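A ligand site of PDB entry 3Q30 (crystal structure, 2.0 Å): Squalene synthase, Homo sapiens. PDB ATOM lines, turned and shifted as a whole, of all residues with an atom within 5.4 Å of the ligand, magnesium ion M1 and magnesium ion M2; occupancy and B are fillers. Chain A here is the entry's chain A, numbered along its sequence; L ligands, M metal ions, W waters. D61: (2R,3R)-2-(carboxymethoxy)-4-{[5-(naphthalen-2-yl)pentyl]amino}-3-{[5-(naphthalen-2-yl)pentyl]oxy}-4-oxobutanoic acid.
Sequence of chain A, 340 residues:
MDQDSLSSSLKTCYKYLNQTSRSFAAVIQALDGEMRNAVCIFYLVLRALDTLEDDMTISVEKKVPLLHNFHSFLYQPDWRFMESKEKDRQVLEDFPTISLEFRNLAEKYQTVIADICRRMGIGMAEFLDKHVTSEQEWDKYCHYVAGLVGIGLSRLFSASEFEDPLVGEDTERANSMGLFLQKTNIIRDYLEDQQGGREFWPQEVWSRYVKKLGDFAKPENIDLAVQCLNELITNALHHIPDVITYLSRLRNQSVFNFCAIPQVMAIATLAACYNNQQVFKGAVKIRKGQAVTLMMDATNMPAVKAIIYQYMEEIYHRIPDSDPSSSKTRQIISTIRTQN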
ATOM      1  N   ILE A  28      -1.371  11.836 -33.611  1.00  0.00           N
ATOM      2  CA  ILE A  28      -2.819  11.714 -33.749  1.00  0.00           C
ATOM      3  C   ILE A  28      -3.210  11.346 -35.195  1.00  0.00           C
ATOM      4  O   ILE A  28      -3.981  10.422 -35.417  1.00  0.00           O
ATOM      5  CB  ILE A  28      -3.587  12.979 -33.229  1.00  0.00           C
ATOM      6  CG1 ILE A  28      -3.436  13.062 -31.700  1.00  0.00           C
ATOM      7  CG2 ILE A  28      -5.077  12.912 -33.634  1.00  0.00           C
ATOM      8  CD1 ILE A  28      -3.968  14.332 -31.034  1.00  0.00           C
ATOM      9  N   VAL A  39     -10.041  10.963 -31.769  1.00  0.00           N
ATOM     10  CA  VAL A  39      -9.020  11.515 -30.879  1.00  0.00           C
ATOM     11  C   VAL A  39      -8.771  12.975 -31.276  1.00  0.00           C
ATOM     12  O   VAL A  39      -8.566  13.843 -30.404  1.00  0.00           O
ATOM     13  CB  VAL A  39      -7.708  10.614 -30.882  1.00  0.00           C
ATOM     14  CG1 VAL A  39      -6.507  11.344 -30.285  1.00  0.00           C
ATOM     15  CG2 VAL A  39      -7.940   9.298 -30.204  1.00  0.00           C
ATOM     16  N   PHE A  42     -11.656  14.744 -29.631  1.00  0.00           N
ATOM     17  CA  PHE A  42     -11.491  14.684 -28.144  1.00  0.00           C
ATOM     18  C   PHE A  42     -10.459  15.714 -27.646  1.00  0.00           C
ATOM     19  O   PHE A  42     -10.598  16.336 -26.560  1.00  0.00           O
ATOM     20  CB  PHE A  42     -11.019  13.272 -27.770  1.00  0.00           C
ATOM     21  CG  PHE A  42     -11.010  12.983 -26.288  1.00  0.00           C
ATOM     22  CD1 PHE A  42     -10.062  12.124 -25.771  1.00  0.00           C
ATOM     23  CD2 PHE A  42     -12.000  13.475 -25.448  1.00  0.00           C
ATOM     24  CE1 PHE A  42     -10.049  11.824 -24.403  1.00  0.00           C
ATOM     25  CE2 PHE A  42     -11.986  13.168 -24.087  1.00  0.00           C
ATOM     26  CZ  PHE A  42     -11.018  12.338 -23.582  1.00  0.00           C
ATOM     27  N   TYR A  43      -9.390  15.817 -28.426  1.00  0.00           N
ATOM     28  CA  TYR A  43      -8.342  16.776 -28.138  1.00  0.00           C
ATOM     29  C   TYR A  43      -8.887  18.194 -28.133  1.00  0.00           C
ATOM     30  O   TYR A  43      -8.709  18.926 -27.161  1.00  0.00           O
ATOM     31  CB  TYR A  43      -7.190  16.681 -29.136  1.00  0.00           C
ATOM     32  CG  TYR A  43      -6.123  17.681 -28.787  1.00  0.00           C
ATOM     33  CD1 TYR A  43      -6.137  18.967 -29.351  1.00  0.00           C
ATOM     34  CD2 TYR A  43      -5.155  17.382 -27.820  1.00  0.00           C
ATOM     35  CE1 TYR A  43      -5.197  19.907 -28.986  1.00  0.00           C
ATOM     36  CE2 TYR A  43      -4.195  18.335 -27.437  1.00  0.00           C
ATOM     37  CZ  TYR A  43      -4.236  19.585 -28.038  1.00  0.00           C
ATOM     38  OH  TYR A  43      -3.304  20.531 -27.708  1.00  0.00           O
ATOM     39  N   LEU A  46     -11.352  19.014 -25.341  1.00  0.00           N
ATOM     40  CA  LEU A  46     -10.797  19.197 -23.991  1.00  0.00           C
ATOM     41  C   LEU A  46      -9.869  20.385 -23.938  1.00  0.00           C
ATOM     42  O   LEU A  46      -9.754  21.022 -22.881  1.00  0.00           O
ATOM     43  CB  LEU A  46     -10.076  17.955 -23.477  1.00  0.00           C
ATOM     44  CG  LEU A  46     -10.974  16.740 -23.290  1.00  0.00           C
ATOM     45  CD1 LEU A  46     -10.108  15.602 -22.861  1.00  0.00           C
ATOM     46  CD2 LEU A  46     -12.132  16.979 -22.265  1.00  0.00           C
ATOM     47  N   ARG A  47      -9.232  20.711 -25.051  1.00  0.00           N
ATOM     48  CA  ARG A  47      -8.463  21.968 -25.123  1.00  0.00           C
ATOM     49  C   ARG A  47      -9.362  23.200 -25.047  1.00  0.00           C
ATOM     50  O   ARG A  47      -8.959  24.199 -24.448  1.00  0.00           O
ATOM     51  CB  ARG A  47      -7.554  22.022 -26.349  1.00  0.00           C
ATOM     52  CG  ARG A  47      -6.399  23.055 -26.288  1.00  0.00           C
ATOM     53  CD  ARG A  47      -5.610  23.115 -24.960  1.00  0.00           C
ATOM     54  NE  ARG A  47      -4.746  21.955 -24.817  1.00  0.00           N
ATOM     55  CZ  ARG A  47      -4.279  21.461 -23.659  1.00  0.00           C
ATOM     56  NH1 ARG A  47      -4.584  22.018 -22.486  1.00  0.00           N
ATOM     57  NH2 ARG A  47      -3.492  20.394 -23.684  1.00  0.00           N
ATOM     58  N   ASP A  50     -10.329  23.378 -21.427  1.00  0.00           N
ATOM     59  CA  ASP A  50      -9.186  23.887 -20.636  1.00  0.00           C
ATOM     60  C   ASP A  50      -8.902  25.383 -20.896  1.00  0.00           C
ATOM     61  O   ASP A  50      -8.386  26.090 -20.031  1.00  0.00           O
ATOM     62  CB  ASP A  50      -7.908  23.100 -20.880  1.00  0.00           C
ATOM     63  CG  ASP A  50      -6.802  23.535 -19.937  1.00  0.00           C
ATOM     64  OD1 ASP A  50      -6.996  23.503 -18.698  1.00  0.00           O
ATOM     65  OD2 ASP A  50      -5.742  23.938 -20.450  1.00  0.00           O
ATOM     66  N   GLU A  53     -11.075  27.104 -18.597  1.00  0.00           N
ATOM     67  CA  GLU A  53     -10.538  26.921 -17.242  1.00  0.00           C
ATOM     68  C   GLU A  53      -9.304  27.802 -16.984  1.00  0.00           C
ATOM     69  O   GLU A  53      -9.189  28.380 -15.911  1.00  0.00           O
ATOM     70  CB  GLU A  53     -10.182  25.434 -16.991  1.00  0.00           C
ATOM     71  CG  GLU A  53     -10.036  25.118 -15.495  1.00  0.00           C
ATOM     72  CD  GLU A  53      -8.704  24.500 -15.157  1.00  0.00           C
ATOM     73  OE1 GLU A  53      -7.758  24.781 -15.913  1.00  0.00           O
ATOM     74  OE2 GLU A  53      -8.589  23.747 -14.148  1.00  0.00           O
ATOM     75  N   ASP A  54      -8.405  27.905 -17.951  1.00  0.00           N
ATOM     76  CA  ASP A  54      -7.168  28.673 -17.805  1.00  0.00           C
ATOM     77  C   ASP A  54      -7.436  30.179 -17.828  1.00  0.00           C
ATOM     78  O   ASP A  54      -6.627  30.975 -17.366  1.00  0.00           O
ATOM     79  CB  ASP A  54      -6.203  28.313 -18.931  1.00  0.00           C
ATOM     80  CG  ASP A  54      -5.565  26.946 -18.737  1.00  0.00           C
ATOM     81  OD1 ASP A  54      -5.794  26.306 -17.694  1.00  0.00           O
ATOM     82  OD2 ASP A  54      -4.858  26.507 -19.659  1.00  0.00           O
ATOM     83  N   MET A 120     -14.463  15.892 -15.975  1.00  0.00           N
ATOM     84  CA  MET A 120     -13.369  16.856 -15.896  1.00  0.00           C
ATOM     85  C   MET A 120     -13.903  18.237 -15.533  1.00  0.00           C
ATOM     86  O   MET A 120     -13.254  18.994 -14.785  1.00  0.00           O
ATOM     87  CB  MET A 120     -12.615  16.928 -17.253  1.00  0.00           C
ATOM     88  CG  MET A 120     -11.495  18.013 -17.302  1.00  0.00           C
ATOM     89  SD  MET A 120     -10.437  17.978 -18.788  1.00  0.00           S
ATOM     90  CE  MET A 120     -10.098  16.171 -18.871  1.00  0.00           C
ATOM     91  N   MET A 124     -12.547  20.336 -12.502  1.00  0.00           N
ATOM     92  CA  MET A 124     -11.952  21.627 -12.725  1.00  0.00           C
ATOM     93  C   MET A 124     -12.689  22.693 -11.884  1.00  0.00           C
ATOM     94  O   MET A 124     -12.053  23.531 -11.257  1.00  0.00           O
ATOM     95  CB  MET A 124     -12.004  21.992 -14.202  1.00  0.00           C
ATOM     96  CG  MET A 124     -10.888  21.359 -15.046  1.00  0.00           C
ATOM     97  SD  MET A 124     -11.297  21.737 -16.728  1.00  0.00           S
ATOM     98  CE  MET A 124      -9.739  21.314 -17.587  1.00  0.00           C
ATOM     99  N   TYR A 141      -6.588  16.424  -8.297  1.00  0.00           N
ATOM    100  CA  TYR A 141      -6.433  17.426  -9.335  1.00  0.00           C
ATOM    101  C   TYR A 141      -5.870  16.815 -10.638  1.00  0.00           C
ATOM    102  O   TYR A 141      -6.477  16.985 -11.693  1.00  0.00           O
ATOM    103  CB  TYR A 141      -5.561  18.623  -8.864  1.00  0.00           C
ATOM    104  CG  TYR A 141      -5.250  19.584  -9.986  1.00  0.00           C
ATOM    105  CD1 TYR A 141      -6.189  20.567 -10.370  1.00  0.00           C
ATOM    106  CD2 TYR A 141      -4.051  19.502 -10.698  1.00  0.00           C
ATOM    107  CE1 TYR A 141      -5.928  21.430 -11.402  1.00  0.00           C
ATOM    108  CE2 TYR A 141      -3.788  20.351 -11.744  1.00  0.00           C
ATOM    109  CZ  TYR A 141      -4.739  21.323 -12.091  1.00  0.00           C
ATOM    110  OH  TYR A 141      -4.472  22.195 -13.131  1.00  0.00           O
ATOM    111  N   VAL A 145      -7.723  16.582 -14.442  1.00  0.00           N
ATOM    112  CA  VAL A 145      -7.295  17.328 -15.622  1.00  0.00           C
ATOM    113  C   VAL A 145      -6.465  16.506 -16.607  1.00  0.00           C
ATOM    114  O   VAL A 145      -6.281  16.916 -17.752  1.00  0.00           O
ATOM    115  CB  VAL A 145      -6.536  18.695 -15.272  1.00  0.00           C
ATOM    116  CG1 VAL A 145      -7.411  19.572 -14.331  1.00  0.00           C
ATOM    117  CG2 VAL A 145      -5.151  18.447 -14.670  1.00  0.00           C
ATOM    118  N   ALA A 146      -5.970  15.349 -16.157  1.00  0.00           N
ATOM    119  CA  ALA A 146      -5.035  14.560 -16.966  1.00  0.00           C
ATOM    120  C   ALA A 146      -5.331  13.044 -16.926  1.00  0.00           C
ATOM    121  O   ALA A 146      -5.273  12.338 -17.954  1.00  0.00           O
ATOM    122  CB  ALA A 146      -3.603  14.822 -16.506  1.00  0.00           C
ATOM    123  N   VAL A 149      -8.175  12.191 -19.120  1.00  0.00           N
ATOM    124  CA  VAL A 149      -7.785  12.153 -20.563  1.00  0.00           C
ATOM    125  C   VAL A 149      -7.278  10.749 -20.935  1.00  0.00           C
ATOM    126  O   VAL A 149      -7.723  10.154 -21.930  1.00  0.00           O
ATOM    127  CB  VAL A 149      -6.705  13.184 -20.928  1.00  0.00           C
ATOM    128  CG1 VAL A 149      -6.402  13.123 -22.485  1.00  0.00           C
ATOM    129  CG2 VAL A 149      -7.180  14.568 -20.590  1.00  0.00           C
ATOM    130  N   GLY A 150      -6.387  10.197 -20.107  1.00  0.00           N
ATOM    131  CA  GLY A 150      -5.965   8.791 -20.248  1.00  0.00           C
ATOM    132  C   GLY A 150      -7.125   7.822 -20.288  1.00  0.00           C
ATOM    133  O   GLY A 150      -7.160   6.877 -21.108  1.00  0.00           O
ATOM    134  N   LEU A 153      -9.170   8.375 -23.632  1.00  0.00           N
ATOM    135  CA  LEU A 153      -8.407   7.810 -24.747  1.00  0.00           C
ATOM    136  C   LEU A 153      -8.459   6.307 -24.734  1.00  0.00           C
ATOM    137  O   LEU A 153      -8.752   5.662 -25.790  1.00  0.00           O
ATOM    138  CB  LEU A 153      -6.941   8.278 -24.706  1.00  0.00           C
ATOM    139  CG  LEU A 153      -6.778   9.763 -25.010  1.00  0.00           C
ATOM    140  CD1 LEU A 153      -5.376  10.187 -24.569  1.00  0.00           C
ATOM    141  CD2 LEU A 153      -6.962   9.980 -26.526  1.00  0.00           C
ATOM    142  N   PHE A 157      -9.844   3.652 -27.662  1.00  0.00           N
ATOM    143  CA  PHE A 157      -9.067   2.529 -28.193  1.00  0.00           C
ATOM    144  C   PHE A 157      -9.898   1.277 -28.103  1.00  0.00           C
ATOM    145  O   PHE A 157      -9.986   0.550 -29.099  1.00  0.00           O
ATOM    146  CB  PHE A 157      -7.690   2.328 -27.498  1.00  0.00           C
ATOM    147  CG  PHE A 157      -6.785   3.591 -27.451  1.00  0.00           C
ATOM    148  CD1 PHE A 157      -5.904   3.750 -26.392  1.00  0.00           C
ATOM    149  CD2 PHE A 157      -6.802   4.563 -28.437  1.00  0.00           C
ATOM    150  CE1 PHE A 157      -5.058   4.840 -26.309  1.00  0.00           C
ATOM    151  CE2 PHE A 157      -5.959   5.697 -28.355  1.00  0.00           C
ATOM    152  CZ  PHE A 157      -5.090   5.808 -27.264  1.00  0.00           C
ATOM    153  N   ALA A 174      -4.566   3.697 -16.890  1.00  0.00           N
ATOM    154  CA  ALA A 174      -4.830   4.844 -17.723  1.00  0.00           C
ATOM    155  C   ALA A 174      -4.721   6.142 -16.916  1.00  0.00           C
ATOM    156  O   ALA A 174      -4.183   7.115 -17.395  1.00  0.00           O
ATOM    157  CB  ALA A 174      -6.210   4.734 -18.354  1.00  0.00           C
ATOM    158  N   MET A 177      -1.038   6.986 -16.508  1.00  0.00           N
ATOM    159  CA  MET A 177      -0.474   7.581 -17.708  1.00  0.00           C
ATOM    160  C   MET A 177      -0.611   9.110 -17.725  1.00  0.00           C
ATOM    161  O   MET A 177       0.321   9.827 -18.136  1.00  0.00           O
ATOM    162  CB  MET A 177      -1.151   7.059 -18.995  1.00  0.00           C
ATOM    163  CG  MET A 177      -0.970   5.558 -19.280  1.00  0.00           C
ATOM    164  SD  MET A 177       0.662   5.174 -19.959  1.00  0.00           S
ATOM    165  CE  MET A 177       0.514   5.869 -21.613  1.00  0.00           C
ATOM    166  N   GLY A 178      -1.808   9.578 -17.373  1.00  0.00           N
ATOM    167  CA  GLY A 178      -2.072  11.050 -17.432  1.00  0.00           C
ATOM    168  C   GLY A 178      -1.406  11.755 -16.255  1.00  0.00           C
ATOM    169  O   GLY A 178      -0.890  12.836 -16.380  1.00  0.00           O
ATOM    170  N   LEU A 181       2.387  12.419 -16.959  1.00  0.00           N
ATOM    171  CA  LEU A 181       2.574  13.536 -17.869  1.00  0.00           C
ATOM    172  C   LEU A 181       2.306  14.847 -17.199  1.00  0.00           C
ATOM    173  O   LEU A 181       3.047  15.804 -17.389  1.00  0.00           O
ATOM    174  CB  LEU A 181       1.690  13.388 -19.107  1.00  0.00           C
ATOM    175  CG  LEU A 181       1.950  12.171 -20.022  1.00  0.00           C
ATOM    176  CD1 LEU A 181       0.954  12.203 -21.237  1.00  0.00           C
ATOM    177  CD2 LEU A 181       3.426  12.229 -20.490  1.00  0.00           C
ATOM    178  N   GLN A 182       1.201  14.911 -16.459  1.00  0.00           N
ATOM    179  CA  GLN A 182       0.788  16.167 -15.864  1.00  0.00           C
ATOM    180  C   GLN A 182       1.693  16.588 -14.707  1.00  0.00           C
ATOM    181  O   GLN A 182       1.989  17.753 -14.560  1.00  0.00           O
ATOM    182  CB  GLN A 182      -0.684  16.079 -15.367  1.00  0.00           C
ATOM    183  CG  GLN A 182      -1.177  17.353 -14.657  1.00  0.00           C
ATOM    184  CD  GLN A 182      -1.509  18.476 -15.615  1.00  0.00           C
ATOM    185  OE1 GLN A 182      -1.499  18.299 -16.811  1.00  0.00           O
ATOM    186  NE2 GLN A 182      -1.829  19.642 -15.062  1.00  0.00           N
ATOM    187  N   ASN A 185       4.976  17.978 -16.129  1.00  0.00           N
ATOM    188  CA  ASN A 185       4.696  19.310 -16.627  1.00  0.00           C
ATOM    189  C   ASN A 185       4.666  20.292 -15.459  1.00  0.00           C
ATOM    190  O   ASN A 185       5.335  21.305 -15.488  1.00  0.00           O
ATOM    191  CB  ASN A 185       3.344  19.241 -17.392  1.00  0.00           C
ATOM    192  CG  ASN A 185       3.056  20.454 -18.194  1.00  0.00           C
ATOM    193  OD1 ASN A 185       3.717  20.739 -19.182  1.00  0.00           O
ATOM    194  ND2 ASN A 185       1.973  21.146 -17.838  1.00  0.00           N
ATOM    195  N   TYR A 246       0.739  -0.392 -18.704  1.00  0.00           N
ATOM    196  CA  TYR A 246      -0.224   0.128 -19.634  1.00  0.00           C
ATOM    197  C   TYR A 246       0.272  -0.093 -21.084  1.00  0.00           C
ATOM    198  O   TYR A 246      -0.449  -0.616 -21.969  1.00  0.00           O
ATOM    199  CB  TYR A 246      -0.473   1.655 -19.395  1.00  0.00           C
ATOM    200  CG  TYR A 246      -1.533   2.206 -20.338  1.00  0.00           C
ATOM    201  CD1 TYR A 246      -1.183   2.666 -21.599  1.00  0.00           C
ATOM    202  CD2 TYR A 246      -2.904   2.247 -19.954  1.00  0.00           C
ATOM    203  CE1 TYR A 246      -2.144   3.171 -22.486  1.00  0.00           C
ATOM    204  CE2 TYR A 246      -3.889   2.759 -20.838  1.00  0.00           C
ATOM    205  CZ  TYR A 246      -3.494   3.210 -22.099  1.00  0.00           C
ATOM    206  OH  TYR A 246      -4.444   3.674 -22.987  1.00  0.00           O
ATOM    207  N   PHE A 258       1.357   6.502 -30.252  1.00  0.00           N
ATOM    208  CA  PHE A 258       0.545   7.575 -29.648  1.00  0.00           C
ATOM    209  C   PHE A 258       0.732   7.661 -28.147  1.00  0.00           C
ATOM    210  O   PHE A 258       0.875   8.740 -27.570  1.00  0.00           O
ATOM    211  CB  PHE A 258      -0.959   7.406 -29.998  1.00  0.00           C
ATOM    212  CG  PHE A 258      -1.848   8.464 -29.374  1.00  0.00           C
ATOM    213  CD1 PHE A 258      -2.621   8.172 -28.253  1.00  0.00           C
ATOM    214  CD2 PHE A 258      -1.909   9.764 -29.887  1.00  0.00           C
ATOM    215  CE1 PHE A 258      -3.483   9.143 -27.682  1.00  0.00           C
ATOM    216  CE2 PHE A 258      -2.730  10.754 -29.288  1.00  0.00           C
ATOM    217  CZ  PHE A 258      -3.519  10.436 -28.185  1.00  0.00           C
ATOM    218  N   CYS A 259       0.781   6.516 -27.506  1.00  0.00           N
ATOM    219  CA  CYS A 259       0.828   6.467 -26.071  1.00  0.00           C
ATOM    220  C   CYS A 259       2.256   6.558 -25.556  1.00  0.00           C
ATOM    221  O   CYS A 259       2.490   7.277 -24.593  1.00  0.00           O
ATOM    222  CB  CYS A 259       0.137   5.200 -25.574  1.00  0.00           C
ATOM    223  SG  CYS A 259      -1.678   5.204 -25.846  1.00  0.00           S
ATOM    224  N   PRO A 262       4.527  10.400 -25.625  1.00  0.00           N
ATOM    225  CA  PRO A 262       4.532  11.442 -24.637  1.00  0.00           C
ATOM    226  C   PRO A 262       5.214  10.913 -23.393  1.00  0.00           C
ATOM    227  O   PRO A 262       5.903  11.692 -22.745  1.00  0.00           O
ATOM    228  CB  PRO A 262       3.032  11.736 -24.373  1.00  0.00           C
ATOM    229  CG  PRO A 262       2.302  11.167 -25.563  1.00  0.00           C
ATOM    230  CD  PRO A 262       3.142   9.972 -25.975  1.00  0.00           C
ATOM    231  N   GLN A 263       5.089   9.610 -23.106  1.00  0.00           N
ATOM    232  CA  GLN A 263       5.718   9.059 -21.903  1.00  0.00           C
ATOM    233  C   GLN A 263       7.242   9.164 -21.964  1.00  0.00           C
ATOM    234  O   GLN A 263       7.865   9.605 -20.997  1.00  0.00           O
ATOM    235  CB  GLN A 263       5.275   7.605 -21.631  1.00  0.00           C
ATOM    236  CG  GLN A 263       3.722   7.504 -21.493  1.00  0.00           C
ATOM    237  CD  GLN A 263       3.233   8.196 -20.234  1.00  0.00           C
ATOM    238  OE1 GLN A 263       3.918   8.159 -19.173  1.00  0.00           O
ATOM    239  NE2 GLN A 263       2.065   8.839 -20.328  1.00  0.00           N
HETATM  240  C1  D61 L   1      -1.964   8.214 -23.695  1.00  0.00           C
HETATM  241  C2  D61 L   1      -1.681   9.142 -24.732  1.00  0.00           C
HETATM  242  C3  D61 L   1      -1.811  10.520 -24.546  1.00  0.00           C
HETATM  243  C4  D61 L   1      -2.224  11.029 -23.281  1.00  0.00           C
HETATM  244  C5  D61 L   1      -2.513  10.091 -22.236  1.00  0.00           C
HETATM  245  C6  D61 L   1      -2.370   8.687 -22.452  1.00  0.00           C
HETATM  246  C7  D61 L   1      -2.958  10.560 -20.979  1.00  0.00           C
HETATM  247  C8  D61 L   1      -3.097  11.927 -20.741  1.00  0.00           C
HETATM  248  C9  D61 L   1      -2.831  12.857 -21.754  1.00  0.00           C
HETATM  249  C10 D61 L   1      -2.390  12.417 -23.039  1.00  0.00           C
HETATM  250  C11 D61 L   1      -2.995  14.332 -21.413  1.00  0.00           C
HETATM  251  C12 D61 L   1      -1.741  14.792 -20.618  1.00  0.00           C
HETATM  252  C13 D61 L   1      -1.733  16.329 -20.459  1.00  0.00           C
HETATM  253  C14 D61 L   1      -0.327  16.942 -20.691  1.00  0.00           C
HETATM  254  C15 D61 L   1      -0.363  18.488 -20.769  1.00  0.00           C
HETATM  255  N16 D61 L   1      -1.278  19.026 -19.727  1.00  0.00           N
HETATM  256  C17 D61 L   1      -2.362  19.744 -20.053  1.00  0.00           C
HETATM  257  O18 D61 L   1      -2.729  19.928 -21.221  1.00  0.00           O
HETATM  258  C19 D61 L   1      -3.158  20.418 -18.949  1.00  0.00           C
HETATM  259  O20 D61 L   1      -4.555  20.503 -19.351  1.00  0.00           O
HETATM  260  C21 D61 L   1      -5.555  19.687 -18.711  1.00  0.00           C
HETATM  261  C22 D61 L   1      -6.871  19.599 -19.482  1.00  0.00           C
HETATM  262  C23 D61 L   1      -6.784  19.697 -21.034  1.00  0.00           C
HETATM  263  C24 D61 L   1      -6.366  18.356 -21.686  1.00  0.00           C
HETATM  264  C25 D61 L   1      -6.225  18.482 -23.191  1.00  0.00           C
HETATM  265  C26 D61 L   1      -5.641  17.289 -23.968  1.00  0.00           C
HETATM  266  C27 D61 L   1      -4.255  17.074 -24.027  1.00  0.00           C
HETATM  267  C28 D61 L   1      -3.740  15.999 -24.759  1.00  0.00           C
HETATM  268  C29 D61 L   1      -4.623  15.166 -25.459  1.00  0.00           C
HETATM  269  C30 D61 L   1      -6.040  15.386 -25.394  1.00  0.00           C
HETATM  270  C31 D61 L   1      -6.539  16.444 -24.657  1.00  0.00           C
HETATM  271  C32 D61 L   1      -6.921  14.553 -26.079  1.00  0.00           C
HETATM  272  C33 D61 L   1      -6.415  13.498 -26.832  1.00  0.00           C
HETATM  273  C34 D61 L   1      -5.042  13.287 -26.896  1.00  0.00           C
HETATM  274  C35 D61 L   1      -4.147  14.102 -26.220  1.00  0.00           C
HETATM  275  C36 D61 L   1      -2.655  21.870 -18.765  1.00  0.00           C
HETATM  276  O37 D61 L   1      -2.835  22.568 -20.048  1.00  0.00           O
HETATM  277  C38 D61 L   1      -1.682  23.064 -20.836  1.00  0.00           C
HETATM  278  C39 D61 L   1      -2.023  24.228 -21.779  1.00  0.00           C
HETATM  279  O40 D61 L   1      -1.250  24.428 -22.755  1.00  0.00           O
HETATM  280  O41 D61 L   1      -3.079  24.903 -21.542  1.00  0.00           O
HETATM  281  C42 D61 L   1      -3.459  22.495 -17.601  1.00  0.00           C
HETATM  282  O43 D61 L   1      -4.185  23.506 -17.808  1.00  0.00           O
HETATM  283  O44 D61 L   1      -3.367  21.931 -16.471  1.00  0.00           O
HETATM  284 MG    MG M   1      -6.119  24.122 -16.953  1.00  0.00          MG
HETATM  285 MG    MG M   2      -3.982  24.602 -19.616  1.00  0.00          MG
HETATM  286  O   HOH W   1      -4.754  25.124 -15.457  1.00  0.00           O
HETATM  287  O   HOH W   2      -4.669  27.975 -21.998  1.00  0.00           O
HETATM  288  O   HOH W   3       1.071   8.988 -23.067  1.00  0.00           O
HETATM  289  O   HOH W   4      -1.937  22.145 -14.007  1.00  0.00           O
HETATM  290  O   HOH W   5      -6.129  22.407 -16.046  1.00  0.00           O
HETATM  291  O   HOH W   6      -2.441  25.508 -18.902  1.00  0.00           O
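OE1 of Gln 182 lies within hydrogen-bond range of N16 of the ligand, at 3.0 Å.
An oxygen (O18) of the ligand sits at hydrogen-bond distance from the guanidinium group (NH2) of Arg 47, 2.6 Å away.
The backbone carbonyl oxygen (O) of Met 177 sits at hydrogen-bond distance from the side-chain amide nitrogen (NE2) of Gln 263.
The side-chain carboxylate (OD2) of Asp 50 lies close to the guanidinium group (NH1) of Arg 47, 3.0 Å away.
Of the 29 residues printed, 3 come within 4 Å of magnesium ion M1.
The nearest printed residue that does not touch magnesium ion M1 is Tyr 141 (4.6 Å).
NH1 of Arg 47 touches magnesium ion M2 (3.9 Å).
Within 4 Å of magnesium ion M2: Arg 47, Asp 50 and Asp 54.
Along chain A the residues within 4 Å of magnesium ion M2 span positions 47 to 54.
Merely in contact with the ligand: Val 145 (3.0 Å), Tyr 43 (3.3 Å), Phe 258 (3.5 Å), Leu 153 (3.5 Å), Tyr 141 (3.5 Å), Gly 150 (3.6 Å), Ala 146 (3.6 Å), Gly 178 (3.6 Å), Val 149 (3.7 Å), Cys 259 (3.7 Å), Leu 46 (3.7 Å), Leu 181 (3.8 Å), Met 124 (3.8 Å), Met 120 (3.98 Å), Phe 42 (3.98 Å) and Met 177 (3.997 Å).
Of the 29 residues printed, 20 come within 4 Å of the ligand.
The nearest printed residue that does not touch the ligand is Val 39 (4.1 Å).
Water W6 is bound to magnesium ion M2.
OD2 of Asp 50 is bound to magnesium ion M2 (2.1 Å).
OD2 of Asp 54 binds magnesium ion M2 (2.1 Å).
Magnesium ion M2 is bound by an oxygen (O43) of the ligand, at 2.1 Å.
Magnesium ion M2 is bound by O41 of the ligand, at 2.1 Å.
Magnesium ion M2 is bound by O37 of the ligand.
Water W5 lies within hydrogen-bond range of O44 of the ligand (2.8 Å), OH of Tyr 141 (3.4 Å) and OE2 of Glu 53 (3.4 Å).
Water W4 lies within hydrogen-bond range of the side-chain hydroxyl (OH) of Tyr 141 (2.7 Å), the side-chain amide nitrogen (NE2) of Gln 182 (2.7 Å) and an oxygen (O44) of the ligand (2.9 Å).
Water W3 lies within hydrogen-bond range of the backbone carbonyl oxygen (O) of Cys 259 (2.7 Å) and the side-chain amide nitrogen (NE2) of Gln 263 (2.9 Å).
Magnesium ion M1 is bound by water W5 (1.9 Å), the side-chain carboxylate (OD1) of Asp 50 (2.0 Å), the side-chain carboxylate (OE1) of Glu 53 (2.0 Å), an oxygen (O43) of the ligand (2.2 Å), water W1 (2.3 Å) and the side-chain carboxylate (OD1) of Asp 54 (2.3 Å).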
